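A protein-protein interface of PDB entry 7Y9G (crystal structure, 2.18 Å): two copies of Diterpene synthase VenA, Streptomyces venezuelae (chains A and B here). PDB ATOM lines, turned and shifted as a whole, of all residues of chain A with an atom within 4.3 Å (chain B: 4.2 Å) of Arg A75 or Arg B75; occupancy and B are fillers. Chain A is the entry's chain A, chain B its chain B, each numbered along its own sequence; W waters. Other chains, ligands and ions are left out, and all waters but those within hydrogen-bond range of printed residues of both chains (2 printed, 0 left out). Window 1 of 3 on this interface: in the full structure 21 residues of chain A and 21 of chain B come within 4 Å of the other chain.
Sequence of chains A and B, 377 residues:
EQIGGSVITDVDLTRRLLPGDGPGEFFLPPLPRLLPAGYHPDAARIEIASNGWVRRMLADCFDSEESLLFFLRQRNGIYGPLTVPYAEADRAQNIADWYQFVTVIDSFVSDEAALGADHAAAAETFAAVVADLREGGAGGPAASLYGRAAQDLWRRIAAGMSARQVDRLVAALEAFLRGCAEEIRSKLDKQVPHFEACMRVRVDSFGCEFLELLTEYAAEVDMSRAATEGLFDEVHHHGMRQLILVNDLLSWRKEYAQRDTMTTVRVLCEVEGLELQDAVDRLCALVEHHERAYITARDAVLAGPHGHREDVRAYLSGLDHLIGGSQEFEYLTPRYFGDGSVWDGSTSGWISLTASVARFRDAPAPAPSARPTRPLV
Ile A48 touches Arg B75, and with the chains exchanged Arg A75 touches Ile B48.
Arg A75 touches its own counterpart, Arg B75.
Positions printed for both chains: 47, 48, 72, 73, 74, 75, 76, 77, 78, 79, 329 and 332.
Of the 3 pairs that touch across the chains among the printed residues, 3 have their exchanged pair printed and touching as well.
The side-chain carboxylate (OE2) of Glu A47 lies within salt-bridge range of the guanidinium group (NE) of Arg A75 (2.8 Å).
OE1 of Glu B47 lies within salt-bridge range of NH2 of Arg B75.
Of the 12 printed residues of chain A, 2 touch a printed residue of chain B.
Printed residues of chain A that touch a printed residue of chain B: Ile A48 and Arg A75.
Hydrophobic or aromatic side chains of chain A within 4 Å of the printed part of chain B: Ile A48.
Printed residues of chain B that touch a printed residue of chain A: Ile B48 and Arg B75.
Hydrophobic or aromatic side chains of chain B that line the printed part of chain A: Ile B48.
Water W2 bridges the side-chain carboxylate of Glu B47 (2.6 Å) and the guanidinium group of Arg A75 (2.8 Å).
Water W1 bridges OE1 of Glu A47 (2.7 Å) and NH2 of Arg B75 (3.0 Å).
NH1 of Arg B75 touches CD1 of Ile A48, at 3.9 Å.
Ile B48 touches Arg A75 (CD1 to NH1, 3.9 Å).
Arg B75 touches two residues of chain A.
Of the printed residues of chain A, Ile B48 touches Arg A75 (3.9 Å).
Of the printed residues of chain B, Ile A48 touches Arg B75.
Arg A73 touches none of the printed residues of chain B.
The nearest printed residue of chain B that does not touch Arg A75 is Glu B47 (4.2 Å).
The nearest residue of chain A that does not touch Arg B75 is Glu A47 (4.1 Å).
The guanidinium group of Arg A75 lies close to the guanidinium group of Arg B75, 3.4 Å away.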
ATOM      1  N   GLU A  47     -12.711  29.408   4.662  1.00  0.00           N
ATOM      2  CA  GLU A  47     -11.295  29.157   4.276  1.00  0.00           C
ATOM      3  C   GLU A  47     -11.031  29.840   2.925  1.00  0.00           C
ATOM      4  O   GLU A  47      -9.996  30.571   2.794  1.00  0.00           O
ATOM      5  CB  GLU A  47     -11.011  27.647   4.203  1.00  0.00           C
ATOM      6  CG  GLU A  47      -9.635  27.324   3.625  1.00  0.00           C
ATOM      7  CD  GLU A  47      -9.328  25.848   3.457  1.00  0.00           C
ATOM      8  OE1 GLU A  47     -10.252  25.046   3.680  1.00  0.00           O
ATOM      9  OE2 GLU A  47      -8.179  25.488   3.030  1.00  0.00           O
ATOM     10  N   ILE A  48     -11.945  29.613   1.973  1.00  0.00           N
ATOM     11  CA  ILE A  48     -11.877  30.176   0.594  1.00  0.00           C
ATOM     12  C   ILE A  48     -11.930  31.704   0.670  1.00  0.00           C
ATOM     13  O   ILE A  48     -11.101  32.354  -0.002  1.00  0.00           O
ATOM     14  CB  ILE A  48     -12.981  29.603  -0.326  1.00  0.00           C
ATOM     15  CG1 ILE A  48     -12.908  28.086  -0.475  1.00  0.00           C
ATOM     16  CG2 ILE A  48     -12.941  30.293  -1.690  1.00  0.00           C
ATOM     17  CD1 ILE A  48     -11.498  27.565  -0.739  1.00  0.00           C
ATOM     18  N   LEU A  72      -1.029  29.548   0.410  1.00  0.00           N
ATOM     19  CA  LEU A  72      -2.485  29.208   0.435  1.00  0.00           C
ATOM     20  C   LEU A  72      -2.705  27.686   0.523  1.00  0.00           C
ATOM     21  O   LEU A  72      -3.693  27.269   1.126  1.00  0.00           O
ATOM     22  CB  LEU A  72      -3.172  29.822  -0.780  1.00  0.00           C
ATOM     23  CG  LEU A  72      -3.114  31.346  -0.830  1.00  0.00           C
ATOM     24  CD1 LEU A  72      -3.812  31.845  -2.078  1.00  0.00           C
ATOM     25  CD2 LEU A  72      -3.744  31.964   0.417  1.00  0.00           C
ATOM     26  N   ARG A  73      -1.809  26.867  -0.037  1.00  0.00           N
ATOM     27  CA  ARG A  73      -1.945  25.398   0.008  1.00  0.00           C
ATOM     28  C   ARG A  73      -1.819  24.909   1.460  1.00  0.00           C
ATOM     29  O   ARG A  73      -2.194  23.752   1.725  1.00  0.00           O
ATOM     30  CB  ARG A  73      -0.942  24.718  -0.926  1.00  0.00           C
ATOM     31  CG  ARG A  73      -1.353  24.688  -2.392  1.00  0.00           C
ATOM     32  CD  ARG A  73      -0.508  23.733  -3.232  1.00  0.00           C
ATOM     33  NE  ARG A  73       0.913  24.076  -3.211  1.00  0.00           N
ATOM     34  CZ  ARG A  73       1.514  24.986  -3.990  1.00  0.00           C
ATOM     35  NH1 ARG A  73       0.846  25.659  -4.908  1.00  0.00           N
ATOM     36  NH2 ARG A  73       2.808  25.198  -3.862  1.00  0.00           N
ATOM     37  N   GLN A  74      -1.310  25.722   2.383  1.00  0.00           N
ATOM     38  CA  GLN A  74      -1.213  25.320   3.816  1.00  0.00           C
ATOM     39  C   GLN A  74      -2.612  25.274   4.458  1.00  0.00           C
ATOM     40  O   GLN A  74      -2.746  24.649   5.562  1.00  0.00           O
ATOM     41  CB  GLN A  74      -0.270  26.260   4.557  1.00  0.00           C
ATOM     42  CG  GLN A  74       1.165  26.175   4.065  1.00  0.00           C
ATOM     43  CD  GLN A  74       2.059  27.156   4.778  1.00  0.00           C
ATOM     44  OE1 GLN A  74       1.713  27.704   5.832  1.00  0.00           O
ATOM     45  NE2 GLN A  74       3.225  27.383   4.198  1.00  0.00           N
ATOM     46  N   ARG A  75      -3.630  25.842   3.791  1.00  0.00           N
ATOM     47  CA  ARG A  75      -5.027  25.826   4.284  1.00  0.00           C
ATOM     48  C   ARG A  75      -5.119  26.495   5.663  1.00  0.00           C
ATOM     49  O   ARG A  75      -5.945  26.078   6.469  1.00  0.00           O
ATOM     50  CB  ARG A  75      -5.509  24.381   4.379  1.00  0.00           C
ATOM     51  CG  ARG A  75      -5.424  23.622   3.065  1.00  0.00           C
ATOM     52  CD  ARG A  75      -6.336  22.417   3.025  1.00  0.00           C
ATOM     53  NE  ARG A  75      -7.694  22.771   3.402  1.00  0.00           N
ATOM     54  CZ  ARG A  75      -8.660  21.881   3.622  1.00  0.00           C
ATOM     55  NH1 ARG A  75      -8.405  20.592   3.495  1.00  0.00           N
ATOM     56  NH2 ARG A  75      -9.881  22.276   3.962  1.00  0.00           N
ATOM     57  N   ASN A  76      -4.325  27.532   5.910  1.00  0.00           N
ATOM     58  CA  ASN A  76      -4.326  28.329   7.171  1.00  0.00           C
ATOM     59  C   ASN A  76      -5.692  28.986   7.381  1.00  0.00           C
ATOM     60  O   ASN A  76      -6.034  29.323   8.544  1.00  0.00           O
ATOM     61  CB  ASN A  76      -3.201  29.363   7.146  1.00  0.00           C
ATOM     62  CG  ASN A  76      -1.845  28.691   7.164  1.00  0.00           C
ATOM     63  OD1 ASN A  76      -1.611  27.802   7.979  1.00  0.00           O
ATOM     64  ND2 ASN A  76      -0.963  29.104   6.269  1.00  0.00           N
ATOM     65  N   GLY A  77      -6.432  29.174   6.293  1.00  0.00           N
ATOM     66  CA  GLY A  77      -7.756  29.804   6.310  1.00  0.00           C
ATOM     67  C   GLY A  77      -8.809  28.978   7.011  1.00  0.00           C
ATOM     68  O   GLY A  77      -9.840  29.576   7.363  1.00  0.00           O
ATOM     69  N   ILE A  78      -8.599  27.667   7.195  1.00  0.00           N
ATOM     70  CA  ILE A  78      -9.556  26.827   7.978  1.00  0.00           C
ATOM     71  C   ILE A  78      -9.159  26.735   9.466  1.00  0.00           C
ATOM     72  O   ILE A  78      -9.973  26.159  10.203  1.00  0.00           O
ATOM     73  CB  ILE A  78      -9.753  25.425   7.371  1.00  0.00           C
ATOM     74  CG1 ILE A  78     -11.082  24.816   7.828  1.00  0.00           C
ATOM     75  CG2 ILE A  78      -8.598  24.507   7.707  1.00  0.00           C
ATOM     76  CD1 ILE A  78     -11.509  23.641   7.042  1.00  0.00           C
ATOM     77  N   TYR A  79      -7.990  27.227   9.919  1.00  0.00           N
ATOM     78  CA  TYR A  79      -7.636  27.285  11.373  1.00  0.00           C
ATOM     79  C   TYR A  79      -8.705  28.061  12.172  1.00  0.00           C
ATOM     80  O   TYR A  79      -9.213  27.570  13.195  1.00  0.00           O
ATOM     81  CB  TYR A  79      -6.271  27.941  11.609  1.00  0.00           C
ATOM     82  CG  TYR A  79      -5.918  28.039  13.063  1.00  0.00           C
ATOM     83  CD1 TYR A  79      -5.584  26.914  13.795  1.00  0.00           C
ATOM     84  CD2 TYR A  79      -5.964  29.244  13.731  1.00  0.00           C
ATOM     85  CE1 TYR A  79      -5.262  26.989  15.142  1.00  0.00           C
ATOM     86  CE2 TYR A  79      -5.646  29.336  15.082  1.00  0.00           C
ATOM     87  CZ  TYR A  79      -5.296  28.204  15.798  1.00  0.00           C
ATOM     88  OH  TYR A  79      -5.019  28.278  17.146  1.00  0.00           O
ATOM     89  N   PHE A 329      -6.393  21.034  13.304  1.00  0.00           N
ATOM     90  CA  PHE A 329      -5.783  21.852  12.214  1.00  0.00           C
ATOM     91  C   PHE A 329      -4.321  21.421  11.976  1.00  0.00           C
ATOM     92  O   PHE A 329      -3.913  21.213  10.823  1.00  0.00           O
ATOM     93  CB  PHE A 329      -5.851  23.363  12.496  1.00  0.00           C
ATOM     94  CG  PHE A 329      -5.077  24.167  11.477  1.00  0.00           C
ATOM     95  CD1 PHE A 329      -5.555  24.319  10.183  1.00  0.00           C
ATOM     96  CD2 PHE A 329      -3.823  24.658  11.763  1.00  0.00           C
ATOM     97  CE1 PHE A 329      -4.804  24.969   9.213  1.00  0.00           C
ATOM     98  CE2 PHE A 329      -3.079  25.320  10.796  1.00  0.00           C
ATOM     99  CZ  PHE A 329      -3.568  25.468   9.521  1.00  0.00           C
ATOM    100  N   LEU A 332      -3.912  18.571   9.961  1.00  0.00           N
ATOM    101  CA  LEU A 332      -4.479  18.811   8.595  1.00  0.00           C
ATOM    102  C   LEU A 332      -3.470  19.521   7.665  1.00  0.00           C
ATOM    103  O   LEU A 332      -3.441  19.201   6.426  1.00  0.00           O
ATOM    104  CB  LEU A 332      -5.782  19.603   8.763  1.00  0.00           C
ATOM    105  CG  LEU A 332      -6.586  19.908   7.498  1.00  0.00           C
ATOM    106  CD1 LEU A 332      -8.073  20.059   7.836  1.00  0.00           C
ATOM    107  CD2 LEU A 332      -6.070  21.173   6.807  1.00  0.00           C
ATOM    108  N   GLU B  47     -14.775  15.858   3.617  1.00  0.00           N
ATOM    109  CA  GLU B  47     -13.688  15.851   2.592  1.00  0.00           C
ATOM    110  C   GLU B  47     -12.507  15.013   3.101  1.00  0.00           C
ATOM    111  O   GLU B  47     -12.142  14.047   2.414  1.00  0.00           O
ATOM    112  CB  GLU B  47     -13.248  17.274   2.278  1.00  0.00           C
ATOM    113  CG  GLU B  47     -12.099  17.341   1.289  1.00  0.00           C
ATOM    114  CD  GLU B  47     -11.632  18.753   1.010  1.00  0.00           C
ATOM    115  OE1 GLU B  47     -12.230  19.710   1.597  1.00  0.00           O
ATOM    116  OE2 GLU B  47     -10.705  18.897   0.188  1.00  0.00           O
ATOM    117  N   ILE B  48     -12.009  15.316   4.303  1.00  0.00           N
ATOM    118  CA  ILE B  48     -10.877  14.606   4.976  1.00  0.00           C
ATOM    119  C   ILE B  48     -11.223  13.118   5.161  1.00  0.00           C
ATOM    120  O   ILE B  48     -10.395  12.262   4.768  1.00  0.00           O
ATOM    121  CB  ILE B  48     -10.514  15.287   6.326  1.00  0.00           C
ATOM    122  CG1 ILE B  48     -10.148  16.772   6.207  1.00  0.00           C
ATOM    123  CG2 ILE B  48      -9.417  14.524   7.049  1.00  0.00           C
ATOM    124  CD1 ILE B  48      -9.091  17.079   5.157  1.00  0.00           C
ATOM    125  N   LEU B  72      -5.973  13.520  -4.505  1.00  0.00           N
ATOM    126  CA  LEU B  72      -6.526  14.049  -3.241  1.00  0.00           C
ATOM    127  C   LEU B  72      -6.468  15.579  -3.240  1.00  0.00           C
ATOM    128  O   LEU B  72      -7.362  16.197  -2.613  1.00  0.00           O
ATOM    129  CB  LEU B  72      -5.793  13.397  -2.063  1.00  0.00           C
ATOM    130  CG  LEU B  72      -6.030  11.893  -1.927  1.00  0.00           C
ATOM    131  CD1 LEU B  72      -5.407  11.379  -0.653  1.00  0.00           C
ATOM    132  CD2 LEU B  72      -7.506  11.549  -1.965  1.00  0.00           C
ATOM    133  N   ARG B  73      -5.525  16.185  -3.964  1.00  0.00           N
ATOM    134  CA  ARG B  73      -5.369  17.661  -3.965  1.00  0.00           C
ATOM    135  C   ARG B  73      -6.478  18.279  -4.806  1.00  0.00           C
ATOM    136  O   ARG B  73      -6.704  19.487  -4.649  1.00  0.00           O
ATOM    137  CB  ARG B  73      -3.994  18.108  -4.457  1.00  0.00           C
ATOM    138  CG  ARG B  73      -2.889  17.931  -3.422  1.00  0.00           C
ATOM    139  CD  ARG B  73      -1.648  18.700  -3.809  1.00  0.00           C
ATOM    140  NE  ARG B  73      -1.088  18.234  -5.072  1.00  0.00           N
ATOM    141  CZ  ARG B  73      -0.190  17.261  -5.218  1.00  0.00           C
ATOM    142  NH1 ARG B  73       0.281  16.601  -4.175  1.00  0.00           N
ATOM    143  NH2 ARG B  73       0.253  16.958  -6.428  1.00  0.00           N
ATOM    144  N   GLN B  74      -7.182  17.483  -5.619  1.00  0.00           N
ATOM    145  CA  GLN B  74      -8.361  17.986  -6.375  1.00  0.00           C
ATOM    146  C   GLN B  74      -9.532  18.272  -5.434  1.00  0.00           C
ATOM    147  O   GLN B  74     -10.461  18.924  -5.882  1.00  0.00           O
ATOM    148  CB  GLN B  74      -8.781  16.990  -7.436  1.00  0.00           C
ATOM    149  CG  GLN B  74      -7.647  16.710  -8.389  1.00  0.00           C
ATOM    150  CD  GLN B  74      -8.069  15.787  -9.499  1.00  0.00           C
ATOM    151  OE1 GLN B  74      -9.230  15.439  -9.626  1.00  0.00           O
ATOM    152  NE2 GLN B  74      -7.103  15.374 -10.302  1.00  0.00           N
ATOM    153  N   ARG B  75      -9.453  17.867  -4.162  1.00  0.00           N
ATOM    154  CA  ARG B  75     -10.489  18.149  -3.138  1.00  0.00           C
ATOM    155  C   ARG B  75     -11.833  17.582  -3.630  1.00  0.00           C
ATOM    156  O   ARG B  75     -12.876  18.197  -3.357  1.00  0.00           O
ATOM    157  CB  ARG B  75     -10.535  19.655  -2.868  1.00  0.00           C
ATOM    158  CG  ARG B  75      -9.213  20.237  -2.378  1.00  0.00           C
ATOM    159  CD  ARG B  75      -9.360  21.595  -1.716  1.00  0.00           C
ATOM    160  NE  ARG B  75     -10.260  21.504  -0.571  1.00  0.00           N
ATOM    161  CZ  ARG B  75     -10.841  22.536   0.025  1.00  0.00           C
ATOM    162  NH1 ARG B  75     -10.544  23.766  -0.354  1.00  0.00           N
ATOM    163  NH2 ARG B  75     -11.683  22.338   1.028  1.00  0.00           N
ATOM    164  N   ASN B  76     -11.820  16.431  -4.303  1.00  0.00           N
ATOM    165  CA  ASN B  76     -13.048  15.814  -4.864  1.00  0.00           C
ATOM    166  C   ASN B  76     -13.950  15.372  -3.711  1.00  0.00           C
ATOM    167  O   ASN B  76     -15.166  15.310  -3.913  1.00  0.00           O
ATOM    168  CB  ASN B  76     -12.754  14.655  -5.820  1.00  0.00           C
ATOM    169  CG  ASN B  76     -12.118  15.111  -7.117  1.00  0.00           C
ATOM    170  OD1 ASN B  76     -12.637  15.997  -7.790  1.00  0.00           O
ATOM    171  ND2 ASN B  76     -11.024  14.474  -7.486  1.00  0.00           N
ATOM    172  N   GLY B  77     -13.379  15.164  -2.528  1.00  0.00           N
ATOM    173  CA  GLY B  77     -14.136  14.767  -1.330  1.00  0.00           C
ATOM    174  C   GLY B  77     -15.183  15.800  -0.935  1.00  0.00           C
ATOM    175  O   GLY B  77     -16.112  15.430  -0.209  1.00  0.00           O
ATOM    176  N   ILE B  78     -15.033  17.065  -1.321  1.00  0.00           N
ATOM    177  CA  ILE B  78     -15.975  18.130  -0.870  1.00  0.00           C
ATOM    178  C   ILE B  78     -17.099  18.305  -1.897  1.00  0.00           C
ATOM    179  O   ILE B  78     -18.030  19.064  -1.587  1.00  0.00           O
ATOM    180  CB  ILE B  78     -15.233  19.448  -0.575  1.00  0.00           C
ATOM    181  CG1 ILE B  78     -15.968  20.278   0.470  1.00  0.00           C
ATOM    182  CG2 ILE B  78     -14.952  20.257  -1.834  1.00  0.00           C
ATOM    183  CD1 ILE B  78     -15.159  21.449   0.965  1.00  0.00           C
ATOM    184  N   TYR B  79     -17.003  17.676  -3.072  1.00  0.00           N
ATOM    185  CA  TYR B  79     -18.067  17.691  -4.111  1.00  0.00           C
ATOM    186  C   TYR B  79     -19.369  17.143  -3.500  1.00  0.00           C
ATOM    187  O   TYR B  79     -20.385  17.853  -3.529  1.00  0.00           O
ATOM    188  CB  TYR B  79     -17.704  16.879  -5.363  1.00  0.00           C
ATOM    189  CG  TYR B  79     -18.842  16.845  -6.345  1.00  0.00           C
ATOM    190  CD1 TYR B  79     -19.239  17.997  -7.001  1.00  0.00           C
ATOM    191  CD2 TYR B  79     -19.580  15.693  -6.564  1.00  0.00           C
ATOM    192  CE1 TYR B  79     -20.316  18.004  -7.870  1.00  0.00           C
ATOM    193  CE2 TYR B  79     -20.669  15.685  -7.425  1.00  0.00           C
ATOM    194  CZ  TYR B  79     -21.041  16.844  -8.079  1.00  0.00           C
ATOM    195  OH  TYR B  79     -22.118  16.863  -8.931  1.00  0.00           O
ATOM    196  N   PHE B 329     -18.433  23.826  -6.561  1.00  0.00           N
ATOM    197  CA  PHE B 329     -17.297  22.873  -6.514  1.00  0.00           C
ATOM    198  C   PHE B 329     -16.369  23.071  -7.719  1.00  0.00           C
ATOM    199  O   PHE B 329     -15.122  22.996  -7.592  1.00  0.00           O
ATOM    200  CB  PHE B 329     -17.746  21.415  -6.476  1.00  0.00           C
ATOM    201  CG  PHE B 329     -16.578  20.478  -6.586  1.00  0.00           C
ATOM    202  CD1 PHE B 329     -15.719  20.303  -5.514  1.00  0.00           C
ATOM    203  CD2 PHE B 329     -16.284  19.849  -7.779  1.00  0.00           C
ATOM    204  CE1 PHE B 329     -14.609  19.475  -5.625  1.00  0.00           C
ATOM    205  CE2 PHE B 329     -15.172  19.024  -7.887  1.00  0.00           C
ATOM    206  CZ  PHE B 329     -14.345  18.821  -6.808  1.00  0.00           C
ATOM    207  N   LEU B 332     -13.933  25.536  -7.446  1.00  0.00           N
ATOM    208  CA  LEU B 332     -13.055  25.332  -6.264  1.00  0.00           C
ATOM    209  C   LEU B 332     -11.876  24.413  -6.658  1.00  0.00           C
ATOM    210  O   LEU B 332     -10.743  24.624  -6.162  1.00  0.00           O
ATOM    211  CB  LEU B 332     -13.922  24.799  -5.111  1.00  0.00           C
ATOM    212  CG  LEU B 332     -13.240  24.528  -3.767  1.00  0.00           C
ATOM    213  CD1 LEU B 332     -14.265  24.452  -2.639  1.00  0.00           C
ATOM    214  CD2 LEU B 332     -12.434  23.242  -3.804  1.00  0.00           C
HETATM  215  O   HOH W   1     -12.223  25.167   1.785  1.00  0.00           O
HETATM  216  O   HOH W   2     -11.341  19.858   4.081  1.00  0.00           O
